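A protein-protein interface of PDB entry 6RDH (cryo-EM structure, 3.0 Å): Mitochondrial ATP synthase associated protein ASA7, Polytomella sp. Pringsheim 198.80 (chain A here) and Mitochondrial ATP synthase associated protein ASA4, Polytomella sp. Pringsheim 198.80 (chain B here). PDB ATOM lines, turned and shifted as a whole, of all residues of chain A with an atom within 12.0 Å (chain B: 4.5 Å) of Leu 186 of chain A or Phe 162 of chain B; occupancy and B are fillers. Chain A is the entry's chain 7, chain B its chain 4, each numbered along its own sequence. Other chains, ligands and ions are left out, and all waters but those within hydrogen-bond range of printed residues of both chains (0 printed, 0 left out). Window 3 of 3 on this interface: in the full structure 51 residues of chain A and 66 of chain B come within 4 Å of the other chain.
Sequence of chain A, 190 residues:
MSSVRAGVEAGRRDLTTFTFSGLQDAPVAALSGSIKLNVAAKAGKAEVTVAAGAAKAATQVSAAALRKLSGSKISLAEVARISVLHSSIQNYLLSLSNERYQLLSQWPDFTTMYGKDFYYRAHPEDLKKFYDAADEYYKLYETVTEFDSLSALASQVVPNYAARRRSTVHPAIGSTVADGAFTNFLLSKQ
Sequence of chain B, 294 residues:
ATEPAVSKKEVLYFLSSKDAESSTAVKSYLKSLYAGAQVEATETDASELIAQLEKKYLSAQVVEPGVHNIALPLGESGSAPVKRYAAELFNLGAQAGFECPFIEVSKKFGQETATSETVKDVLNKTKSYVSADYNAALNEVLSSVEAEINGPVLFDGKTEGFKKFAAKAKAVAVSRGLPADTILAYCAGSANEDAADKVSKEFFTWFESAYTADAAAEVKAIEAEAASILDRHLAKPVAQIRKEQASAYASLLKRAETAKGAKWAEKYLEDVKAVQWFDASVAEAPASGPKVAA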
ATOM      1  N   VAL A 177      -6.592 -27.779  17.353  1.00  0.00           N
ATOM      2  CA  VAL A 177      -7.427 -27.807  16.157  1.00  0.00           C
ATOM      3  C   VAL A 177      -7.349 -26.481  15.421  1.00  0.00           C
ATOM      4  O   VAL A 177      -7.319 -26.448  14.190  1.00  0.00           O
ATOM      5  CB  VAL A 177      -8.881 -28.161  16.512  1.00  0.00           C
ATOM      6  CG1 VAL A 177      -9.689 -28.382  15.266  1.00  0.00           C
ATOM      7  CG2 VAL A 177      -8.934 -29.385  17.358  1.00  0.00           C
ATOM      8  N   ALA A 178      -7.286 -25.372  16.151  1.00  0.00           N
ATOM      9  CA  ALA A 178      -7.185 -24.081  15.484  1.00  0.00           C
ATOM     10  C   ALA A 178      -5.824 -23.892  14.828  1.00  0.00           C
ATOM     11  O   ALA A 178      -5.742 -23.292  13.752  1.00  0.00           O
ATOM     12  CB  ALA A 178      -7.464 -22.953  16.466  1.00  0.00           C
ATOM     13  N   ASP A 179      -4.758 -24.442  15.413  1.00  0.00           N
ATOM     14  CA  ASP A 179      -3.458 -24.360  14.758  1.00  0.00           C
ATOM     15  C   ASP A 179      -3.384 -25.281  13.549  1.00  0.00           C
ATOM     16  O   ASP A 179      -2.777 -24.923  12.536  1.00  0.00           O
ATOM     17  CB  ASP A 179      -2.342 -24.684  15.743  1.00  0.00           C
ATOM     18  CG  ASP A 179      -2.145 -23.595  16.771  1.00  0.00           C
ATOM     19  OD1 ASP A 179      -2.491 -22.433  16.478  1.00  0.00           O
ATOM     20  OD2 ASP A 179      -1.643 -23.896  17.872  1.00  0.00           O
ATOM     21  N   GLY A 180      -4.000 -26.461  13.624  1.00  0.00           N
ATOM     22  CA  GLY A 180      -4.061 -27.328  12.461  1.00  0.00           C
ATOM     23  C   GLY A 180      -4.899 -26.753  11.338  1.00  0.00           C
ATOM     24  O   GLY A 180      -4.576 -26.923  10.158  1.00  0.00           O
ATOM     25  N   ALA A 181      -5.956 -26.030  11.680  1.00  0.00           N
ATOM     26  CA  ALA A 181      -6.740 -25.379  10.648  1.00  0.00           C
ATOM     27  C   ALA A 181      -6.045 -24.155  10.090  1.00  0.00           C
ATOM     28  O   ALA A 181      -6.247 -23.822   8.924  1.00  0.00           O
ATOM     29  CB  ALA A 181      -8.109 -25.006  11.183  1.00  0.00           C
ATOM     30  N   PHE A 182      -5.205 -23.490  10.879  1.00  0.00           N
ATOM     31  CA  PHE A 182      -4.366 -22.443  10.308  1.00  0.00           C
ATOM     32  C   PHE A 182      -3.266 -23.022   9.436  1.00  0.00           C
ATOM     33  O   PHE A 182      -2.811 -22.363   8.498  1.00  0.00           O
ATOM     34  CB  PHE A 182      -3.745 -21.603  11.404  1.00  0.00           C
ATOM     35  CG  PHE A 182      -3.316 -20.268  10.945  1.00  0.00           C
ATOM     36  CD1 PHE A 182      -4.216 -19.429  10.333  1.00  0.00           C
ATOM     37  CD2 PHE A 182      -2.026 -19.836  11.142  1.00  0.00           C
ATOM     38  CE1 PHE A 182      -3.836 -18.181   9.914  1.00  0.00           C
ATOM     39  CE2 PHE A 182      -1.640 -18.589  10.728  1.00  0.00           C
ATOM     40  CZ  PHE A 182      -2.546 -17.761  10.109  1.00  0.00           C
ATOM     41  N   THR A 183      -2.815 -24.233   9.745  1.00  0.00           N
ATOM     42  CA  THR A 183      -1.878 -24.920   8.871  1.00  0.00           C
ATOM     43  C   THR A 183      -2.526 -25.255   7.539  1.00  0.00           C
ATOM     44  O   THR A 183      -1.902 -25.101   6.488  1.00  0.00           O
ATOM     45  CB  THR A 183      -1.368 -26.184   9.551  1.00  0.00           C
ATOM     46  OG1 THR A 183      -0.868 -25.852  10.850  1.00  0.00           O
ATOM     47  CG2 THR A 183      -0.259 -26.814   8.744  1.00  0.00           C
ATOM     48  N   ASN A 184      -3.778 -25.704   7.560  1.00  0.00           N
ATOM     49  CA  ASN A 184      -4.484 -25.943   6.305  1.00  0.00           C
ATOM     50  C   ASN A 184      -4.759 -24.643   5.563  1.00  0.00           C
ATOM     51  O   ASN A 184      -4.621 -24.572   4.340  1.00  0.00           O
ATOM     52  CB  ASN A 184      -5.797 -26.662   6.557  1.00  0.00           C
ATOM     53  CG  ASN A 184      -6.668 -26.680   5.338  1.00  0.00           C
ATOM     54  OD1 ASN A 184      -6.224 -27.060   4.260  1.00  0.00           O
ATOM     55  ND2 ASN A 184      -7.903 -26.230   5.484  1.00  0.00           N
ATOM     56  N   PHE A 185      -5.160 -23.607   6.294  1.00  0.00           N
ATOM     57  CA  PHE A 185      -5.596 -22.369   5.669  1.00  0.00           C
ATOM     58  C   PHE A 185      -4.430 -21.611   5.066  1.00  0.00           C
ATOM     59  O   PHE A 185      -4.557 -21.028   3.986  1.00  0.00           O
ATOM     60  CB  PHE A 185      -6.305 -21.508   6.705  1.00  0.00           C
ATOM     61  CG  PHE A 185      -6.675 -20.151   6.217  1.00  0.00           C
ATOM     62  CD1 PHE A 185      -5.930 -19.042   6.582  1.00  0.00           C
ATOM     63  CD2 PHE A 185      -7.792 -19.975   5.430  1.00  0.00           C
ATOM     64  CE1 PHE A 185      -6.275 -17.798   6.144  1.00  0.00           C
ATOM     65  CE2 PHE A 185      -8.145 -18.729   4.991  1.00  0.00           C
ATOM     66  CZ  PHE A 185      -7.385 -17.641   5.346  1.00  0.00           C
ATOM     67  N   LEU A 186      -3.295 -21.598   5.753  1.00  0.00           N
ATOM     68  CA  LEU A 186      -2.191 -20.763   5.311  1.00  0.00           C
ATOM     69  C   LEU A 186      -1.406 -21.445   4.201  1.00  0.00           C
ATOM     70  O   LEU A 186      -0.886 -20.776   3.305  1.00  0.00           O
ATOM     71  CB  LEU A 186      -1.289 -20.438   6.496  1.00  0.00           C
ATOM     72  CG  LEU A 186      -0.401 -19.222   6.296  1.00  0.00           C
ATOM     73  CD1 LEU A 186      -1.286 -18.012   6.201  1.00  0.00           C
ATOM     74  CD2 LEU A 186       0.562 -19.067   7.434  1.00  0.00           C
ATOM     75  N   LEU A 187      -1.321 -22.773   4.243  1.00  0.00           N
ATOM     76  CA  LEU A 187      -0.639 -23.551   3.219  1.00  0.00           C
ATOM     77  C   LEU A 187      -1.549 -23.966   2.075  1.00  0.00           C
ATOM     78  O   LEU A 187      -1.143 -24.797   1.260  1.00  0.00           O
ATOM     79  CB  LEU A 187      -0.013 -24.801   3.825  1.00  0.00           C
ATOM     80  CG  LEU A 187       0.963 -24.600   4.978  1.00  0.00           C
ATOM     81  CD1 LEU A 187       1.630 -25.913   5.310  1.00  0.00           C
ATOM     82  CD2 LEU A 187       1.983 -23.534   4.663  1.00  0.00           C
ATOM     83  N   SER A 188      -2.767 -23.444   2.006  1.00  0.00           N
ATOM     84  CA  SER A 188      -3.556 -23.567   0.795  1.00  0.00           C
ATOM     85  C   SER A 188      -3.285 -22.354  -0.086  1.00  0.00           C
ATOM     86  O   SER A 188      -2.552 -21.438   0.294  1.00  0.00           O
ATOM     87  CB  SER A 188      -5.040 -23.705   1.119  1.00  0.00           C
ATOM     88  OG  SER A 188      -5.312 -24.937   1.757  1.00  0.00           O
ATOM     89  N   LYS A 189      -3.871 -22.345  -1.282  1.00  0.00           N
ATOM     90  CA  LYS A 189      -3.655 -21.222  -2.185  1.00  0.00           C
ATOM     91  C   LYS A 189      -4.422 -20.008  -1.665  1.00  0.00           C
ATOM     92  O   LYS A 189      -5.600 -19.812  -1.982  1.00  0.00           O
ATOM     93  CB  LYS A 189      -4.033 -21.595  -3.628  1.00  0.00           C
ATOM     94  CG  LYS A 189      -5.322 -22.387  -3.797  1.00  0.00           C
ATOM     95  CD  LYS A 189      -5.696 -22.535  -5.248  1.00  0.00           C
ATOM     96  CE  LYS A 189      -7.147 -22.961  -5.370  1.00  0.00           C
ATOM     97  NZ  LYS A 189      -7.395 -24.274  -4.726  1.00  0.00           N
ATOM     98  N   GLN A 190      -3.725 -19.207  -0.858  1.00  0.00           N
ATOM     99  CA  GLN A 190      -4.219 -18.060  -0.079  1.00  0.00           C
ATOM    100  C   GLN A 190      -5.593 -18.253   0.568  1.00  0.00           C
ATOM    101  O   GLN A 190      -5.965 -19.361   0.950  1.00  0.00           O
ATOM    102  CB  GLN A 190      -4.226 -16.773  -0.933  1.00  0.00           C
ATOM    103  CG  GLN A 190      -5.294 -16.621  -2.024  1.00  0.00           C
ATOM    104  CD  GLN A 190      -6.550 -15.924  -1.533  1.00  0.00           C
ATOM    105  OE1 GLN A 190      -6.494 -15.083  -0.641  1.00  0.00           O
ATOM    106  NE2 GLN A 190      -7.690 -16.278  -2.111  1.00  0.00           N
ATOM    107  N   VAL B 119       1.044 -11.479   4.034  1.00  0.00           N
ATOM    108  CA  VAL B 119       0.888 -12.615   4.935  1.00  0.00           C
ATOM    109  C   VAL B 119       1.136 -12.189   6.379  1.00  0.00           C
ATOM    110  O   VAL B 119       0.519 -12.726   7.309  1.00  0.00           O
ATOM    111  CB  VAL B 119       1.807 -13.762   4.469  1.00  0.00           C
ATOM    112  CG1 VAL B 119       1.774 -14.947   5.406  1.00  0.00           C
ATOM    113  CG2 VAL B 119       1.392 -14.217   3.094  1.00  0.00           C
ATOM    114  N   VAL B 122      -2.227 -11.226   7.587  1.00  0.00           N
ATOM    115  CA  VAL B 122      -3.095 -12.323   8.012  1.00  0.00           C
ATOM    116  C   VAL B 122      -2.599 -12.891   9.335  1.00  0.00           C
ATOM    117  O   VAL B 122      -3.369 -13.480  10.098  1.00  0.00           O
ATOM    118  CB  VAL B 122      -3.240 -13.409   6.922  1.00  0.00           C
ATOM    119  CG1 VAL B 122      -3.316 -12.795   5.542  1.00  0.00           C
ATOM    120  CG2 VAL B 122      -2.194 -14.500   7.012  1.00  0.00           C
ATOM    121  N   LEU B 138       5.586 -18.598  12.994  1.00  0.00           N
ATOM    122  CA  LEU B 138       5.307 -18.162  11.633  1.00  0.00           C
ATOM    123  C   LEU B 138       5.861 -16.775  11.348  1.00  0.00           C
ATOM    124  O   LEU B 138       6.269 -16.506  10.214  1.00  0.00           O
ATOM    125  CB  LEU B 138       3.810 -18.189  11.363  1.00  0.00           C
ATOM    126  CG  LEU B 138       3.239 -19.601  11.302  1.00  0.00           C
ATOM    127  CD1 LEU B 138       1.801 -19.516  10.919  1.00  0.00           C
ATOM    128  CD2 LEU B 138       3.998 -20.469  10.321  1.00  0.00           C
ATOM    129  N   VAL B 153       5.695 -10.246   1.737  1.00  0.00           N
ATOM    130  CA  VAL B 153       5.221 -11.535   1.255  1.00  0.00           C
ATOM    131  C   VAL B 153       3.712 -11.455   1.125  1.00  0.00           C
ATOM    132  O   VAL B 153       2.986 -11.462   2.124  1.00  0.00           O
ATOM    133  CB  VAL B 153       5.633 -12.682   2.191  1.00  0.00           C
ATOM    134  CG1 VAL B 153       5.136 -14.003   1.639  1.00  0.00           C
ATOM    135  CG2 VAL B 153       7.135 -12.698   2.384  1.00  0.00           C
ATOM    136  N   LEU B 154       3.234 -11.344  -0.107  1.00  0.00           N
ATOM    137  CA  LEU B 154       1.812 -11.175  -0.325  1.00  0.00           C
ATOM    138  C   LEU B 154       1.108 -12.522  -0.268  1.00  0.00           C
ATOM    139  O   LEU B 154       1.712 -13.585  -0.430  1.00  0.00           O
ATOM    140  CB  LEU B 154       1.528 -10.490  -1.664  1.00  0.00           C
ATOM    141  CG  LEU B 154       1.582 -11.287  -2.972  1.00  0.00           C
ATOM    142  CD1 LEU B 154       0.807 -10.561  -4.058  1.00  0.00           C
ATOM    143  CD2 LEU B 154       3.002 -11.528  -3.427  1.00  0.00           C
ATOM    144  N   PHE B 155      -0.199 -12.456  -0.031  1.00  0.00           N
ATOM    145  CA  PHE B 155      -1.035 -13.630   0.196  1.00  0.00           C
ATOM    146  C   PHE B 155      -1.634 -14.042  -1.146  1.00  0.00           C
ATOM    147  O   PHE B 155      -2.804 -13.797  -1.443  1.00  0.00           O
ATOM    148  CB  PHE B 155      -2.094 -13.294   1.240  1.00  0.00           C
ATOM    149  CG  PHE B 155      -2.725 -14.480   1.898  1.00  0.00           C
ATOM    150  CD1 PHE B 155      -1.947 -15.432   2.534  1.00  0.00           C
ATOM    151  CD2 PHE B 155      -4.102 -14.597   1.958  1.00  0.00           C
ATOM    152  CE1 PHE B 155      -2.526 -16.509   3.162  1.00  0.00           C
ATOM    153  CE2 PHE B 155      -4.687 -15.669   2.595  1.00  0.00           C
ATOM    154  CZ  PHE B 155      -3.895 -16.627   3.196  1.00  0.00           C
ATOM    155  N   ASP B 156      -0.801 -14.675  -1.976  1.00  0.00           N
ATOM    156  CA  ASP B 156      -1.147 -14.941  -3.369  1.00  0.00           C
ATOM    157  C   ASP B 156      -1.341 -16.423  -3.661  1.00  0.00           C
ATOM    158  O   ASP B 156      -2.395 -16.821  -4.163  1.00  0.00           O
ATOM    159  CB  ASP B 156      -0.069 -14.358  -4.295  1.00  0.00           C
ATOM    160  CG  ASP B 156      -0.194 -14.847  -5.732  1.00  0.00           C
ATOM    161  OD1 ASP B 156       0.730 -15.545  -6.208  1.00  0.00           O
ATOM    162  OD2 ASP B 156      -1.219 -14.545  -6.380  1.00  0.00           O
ATOM    163  N   GLY B 157      -0.350 -17.255  -3.364  1.00  0.00           N
ATOM    164  CA  GLY B 157      -0.418 -18.672  -3.637  1.00  0.00           C
ATOM    165  C   GLY B 157       0.597 -19.165  -4.644  1.00  0.00           C
ATOM    166  O   GLY B 157       0.954 -20.347  -4.606  1.00  0.00           O
ATOM    167  N   THR B 159       3.387 -16.773  -5.833  1.00  0.00           N
ATOM    168  CA  THR B 159       4.590 -15.953  -5.824  1.00  0.00           C
ATOM    169  C   THR B 159       5.729 -16.723  -5.165  1.00  0.00           C
ATOM    170  O   THR B 159       5.499 -17.549  -4.278  1.00  0.00           O
ATOM    171  CB  THR B 159       4.319 -14.640  -5.092  1.00  0.00           C
ATOM    172  OG1 THR B 159       3.051 -14.125  -5.514  1.00  0.00           O
ATOM    173  CG2 THR B 159       5.378 -13.595  -5.418  1.00  0.00           C
ATOM    174  N   GLU B 160       6.961 -16.464  -5.626  1.00  0.00           N
ATOM    175  CA  GLU B 160       8.135 -17.206  -5.168  1.00  0.00           C
ATOM    176  C   GLU B 160       8.398 -16.989  -3.687  1.00  0.00           C
ATOM    177  O   GLU B 160       8.837 -17.915  -2.993  1.00  0.00           O
ATOM    178  CB  GLU B 160       9.368 -16.794  -5.971  1.00  0.00           C
ATOM    179  CG  GLU B 160       9.241 -16.979  -7.471  1.00  0.00           C
ATOM    180  CD  GLU B 160       8.713 -15.734  -8.161  1.00  0.00           C
ATOM    181  OE1 GLU B 160       8.547 -14.704  -7.477  1.00  0.00           O
ATOM    182  OE2 GLU B 160       8.464 -15.783  -9.382  1.00  0.00           O
ATOM    183  N   GLY B 161       8.123 -15.783  -3.190  1.00  0.00           N
ATOM    184  CA  GLY B 161       8.197 -15.544  -1.759  1.00  0.00           C
ATOM    185  C   GLY B 161       7.153 -16.324  -0.987  1.00  0.00           C
ATOM    186  O   GLY B 161       7.445 -16.875   0.074  1.00  0.00           O
ATOM    187  N   PHE B 162       5.937 -16.424  -1.531  1.00  0.00           N
ATOM    188  CA  PHE B 162       4.903 -17.211  -0.868  1.00  0.00           C
ATOM    189  C   PHE B 162       5.203 -18.700  -0.945  1.00  0.00           C
ATOM    190  O   PHE B 162       4.918 -19.436   0.002  1.00  0.00           O
ATOM    191  CB  PHE B 162       3.531 -16.920  -1.469  1.00  0.00           C
ATOM    192  CG  PHE B 162       2.390 -17.469  -0.655  1.00  0.00           C
ATOM    193  CD1 PHE B 162       1.846 -16.729   0.378  1.00  0.00           C
ATOM    194  CD2 PHE B 162       1.869 -18.727  -0.915  1.00  0.00           C
ATOM    195  CE1 PHE B 162       0.802 -17.229   1.130  1.00  0.00           C
ATOM    196  CE2 PHE B 162       0.831 -19.232  -0.166  1.00  0.00           C
ATOM    197  CZ  PHE B 162       0.295 -18.481   0.853  1.00  0.00           C
ATOM    198  N   LYS B 163       5.768 -19.165  -2.061  1.00  0.00           N
ATOM    199  CA  LYS B 163       6.075 -20.586  -2.184  1.00  0.00           C
ATOM    200  C   LYS B 163       7.208 -20.985  -1.252  1.00  0.00           C
ATOM    201  O   LYS B 163       7.121 -22.010  -0.563  1.00  0.00           O
ATOM    202  CB  LYS B 163       6.424 -20.930  -3.630  1.00  0.00           C
ATOM    203  CG  LYS B 163       5.258 -20.827  -4.595  1.00  0.00           C
ATOM    204  CD  LYS B 163       5.669 -21.275  -5.981  1.00  0.00           C
ATOM    205  CE  LYS B 163       6.598 -20.256  -6.615  1.00  0.00           C
ATOM    206  NZ  LYS B 163       6.945 -20.588  -8.017  1.00  0.00           N
ATOM    207  N   LYS B 164       8.255 -20.167  -1.174  1.00  0.00           N
ATOM    208  CA  LYS B 164       9.348 -20.444  -0.257  1.00  0.00           C
ATOM    209  C   LYS B 164       9.013 -20.080   1.182  1.00  0.00           C
ATOM    210  O   LYS B 164       9.758 -20.459   2.089  1.00  0.00           O
ATOM    211  CB  LYS B 164      10.613 -19.706  -0.695  1.00  0.00           C
ATOM    212  CG  LYS B 164      10.671 -18.248  -0.295  1.00  0.00           C
ATOM    213  CD  LYS B 164      11.923 -17.599  -0.856  1.00  0.00           C
ATOM    214  CE  LYS B 164      13.166 -18.212  -0.242  1.00  0.00           C
ATOM    215  NZ  LYS B 164      13.248 -17.950   1.219  1.00  0.00           N
ATOM    216  N   PHE B 165       7.918 -19.352   1.413  1.00  0.00           N
ATOM    217  CA  PHE B 165       7.419 -19.171   2.768  1.00  0.00           C
ATOM    218  C   PHE B 165       6.618 -20.382   3.215  1.00  0.00           C
ATOM    219  O   PHE B 165       6.781 -20.858   4.340  1.00  0.00           O
ATOM    220  CB  PHE B 165       6.556 -17.911   2.852  1.00  0.00           C
ATOM    221  CG  PHE B 165       5.775 -17.802   4.128  1.00  0.00           C
ATOM    222  CD1 PHE B 165       6.408 -17.454   5.309  1.00  0.00           C
ATOM    223  CD2 PHE B 165       4.410 -18.052   4.153  1.00  0.00           C
ATOM    224  CE1 PHE B 165       5.696 -17.355   6.491  1.00  0.00           C
ATOM    225  CE2 PHE B 165       3.703 -17.965   5.332  1.00  0.00           C
ATOM    226  CZ  PHE B 165       4.346 -17.611   6.499  1.00  0.00           C
ATOM    227  N   ALA B 166       5.727 -20.869   2.350  1.00  0.00           N
ATOM    228  CA  ALA B 166       4.903 -22.023   2.677  1.00  0.00           C
ATOM    229  C   ALA B 166       5.729 -23.292   2.788  1.00  0.00           C
ATOM    230  O   ALA B 166       5.406 -24.162   3.600  1.00  0.00           O
ATOM    231  CB  ALA B 166       3.807 -22.201   1.629  1.00  0.00           C
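The side-chain carboxylate (OD1) of Asp 156 of chain B lies within hydrogen-bond range of the side-chain hydroxyl (OG1) of Thr 159 of chain B, 2.8 Å away.
Among the printed residues, merely in contact across the chains: Phe 182 of chain A with Leu 138 of chain B (3.6 Å), Phe 185 of chain A with Phe 155 of chain B (3.97 Å), Leu 186 of chain A with Val 122 of chain B (3.7 Å), Leu 186 of chain A with Leu 138 of chain B (3.7 Å), Leu 186 of chain A with Phe 155 of chain B (3.6 Å), Leu 186 of chain A with Phe 162 of chain B (3.6 Å), Leu 186 of chain A with Phe 165 of chain B (3.9 Å), Leu 187 of chain A with Ala 166 of chain B (3.6 Å), Gln 190 of chain A with Phe 155 of chain B (3.3 Å) and Gln 190 of chain A with Asp 156 of chain B (3.6 Å).
Printed residues of chain B within 4 Å of Phe 182 of chain A: Leu 138.
Of the printed residues of chain B, Phe 185 of chain A touches Phe 155 (3.97 Å).
Of chain B, only Val 122, Leu 138, Phe 155, Phe 162 and Phe 165 come within 4 Å of Leu 186 of chain A.
Of the printed residues of chain B, Leu 187 of chain A touches Ala 166.
No residue of chain A comes within 4 Å of Val 119 of chain B.
Of the printed residues of chain A, Val 122 of chain B touches Leu 186.
Leu 138 of chain B touches just these residues of chain A: Phe 182 (3.6 Å) and Leu 186 (3.7 Å).
No residue of chain A comes within 4 Å of Val 153 of chain B.
No residue of chain A comes within 4 Å of Leu 154 of chain B.
Of chain A, only Phe 185 (3.97 Å), Leu 186 (3.6 Å) and Gln 190 (3.3 Å) come within 4 Å of Phe 155 of chain B.
Asp 156 of chain B touches just one residue of chain A: Gln 190 (3.6 Å).
No residue of chain A comes within 4 Å of Thr 159 of chain B.
Gly 161 of chain B touches none of the printed residues of chain A.
Phe 162 of chain B touches one residue of chain A.
No residue of chain A comes within 4 Å of Lys 163 of chain B.
Ala 166 of chain B touches one residue of chain A.
Of the 14 printed residues of chain A, 5 touch a printed residue of chain B.
Hydrophobic or aromatic side chains of chain A that line the printed part of chain B: Phe 182, Phe 185, Leu 186 and Leu 187.
Among the printed residues, 10 pairs touch across the chains.
Among the printed residues, no Asp or Glu carboxylate lies within 4 Å of a Lys or Arg side-chain nitrogen of the other chain.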
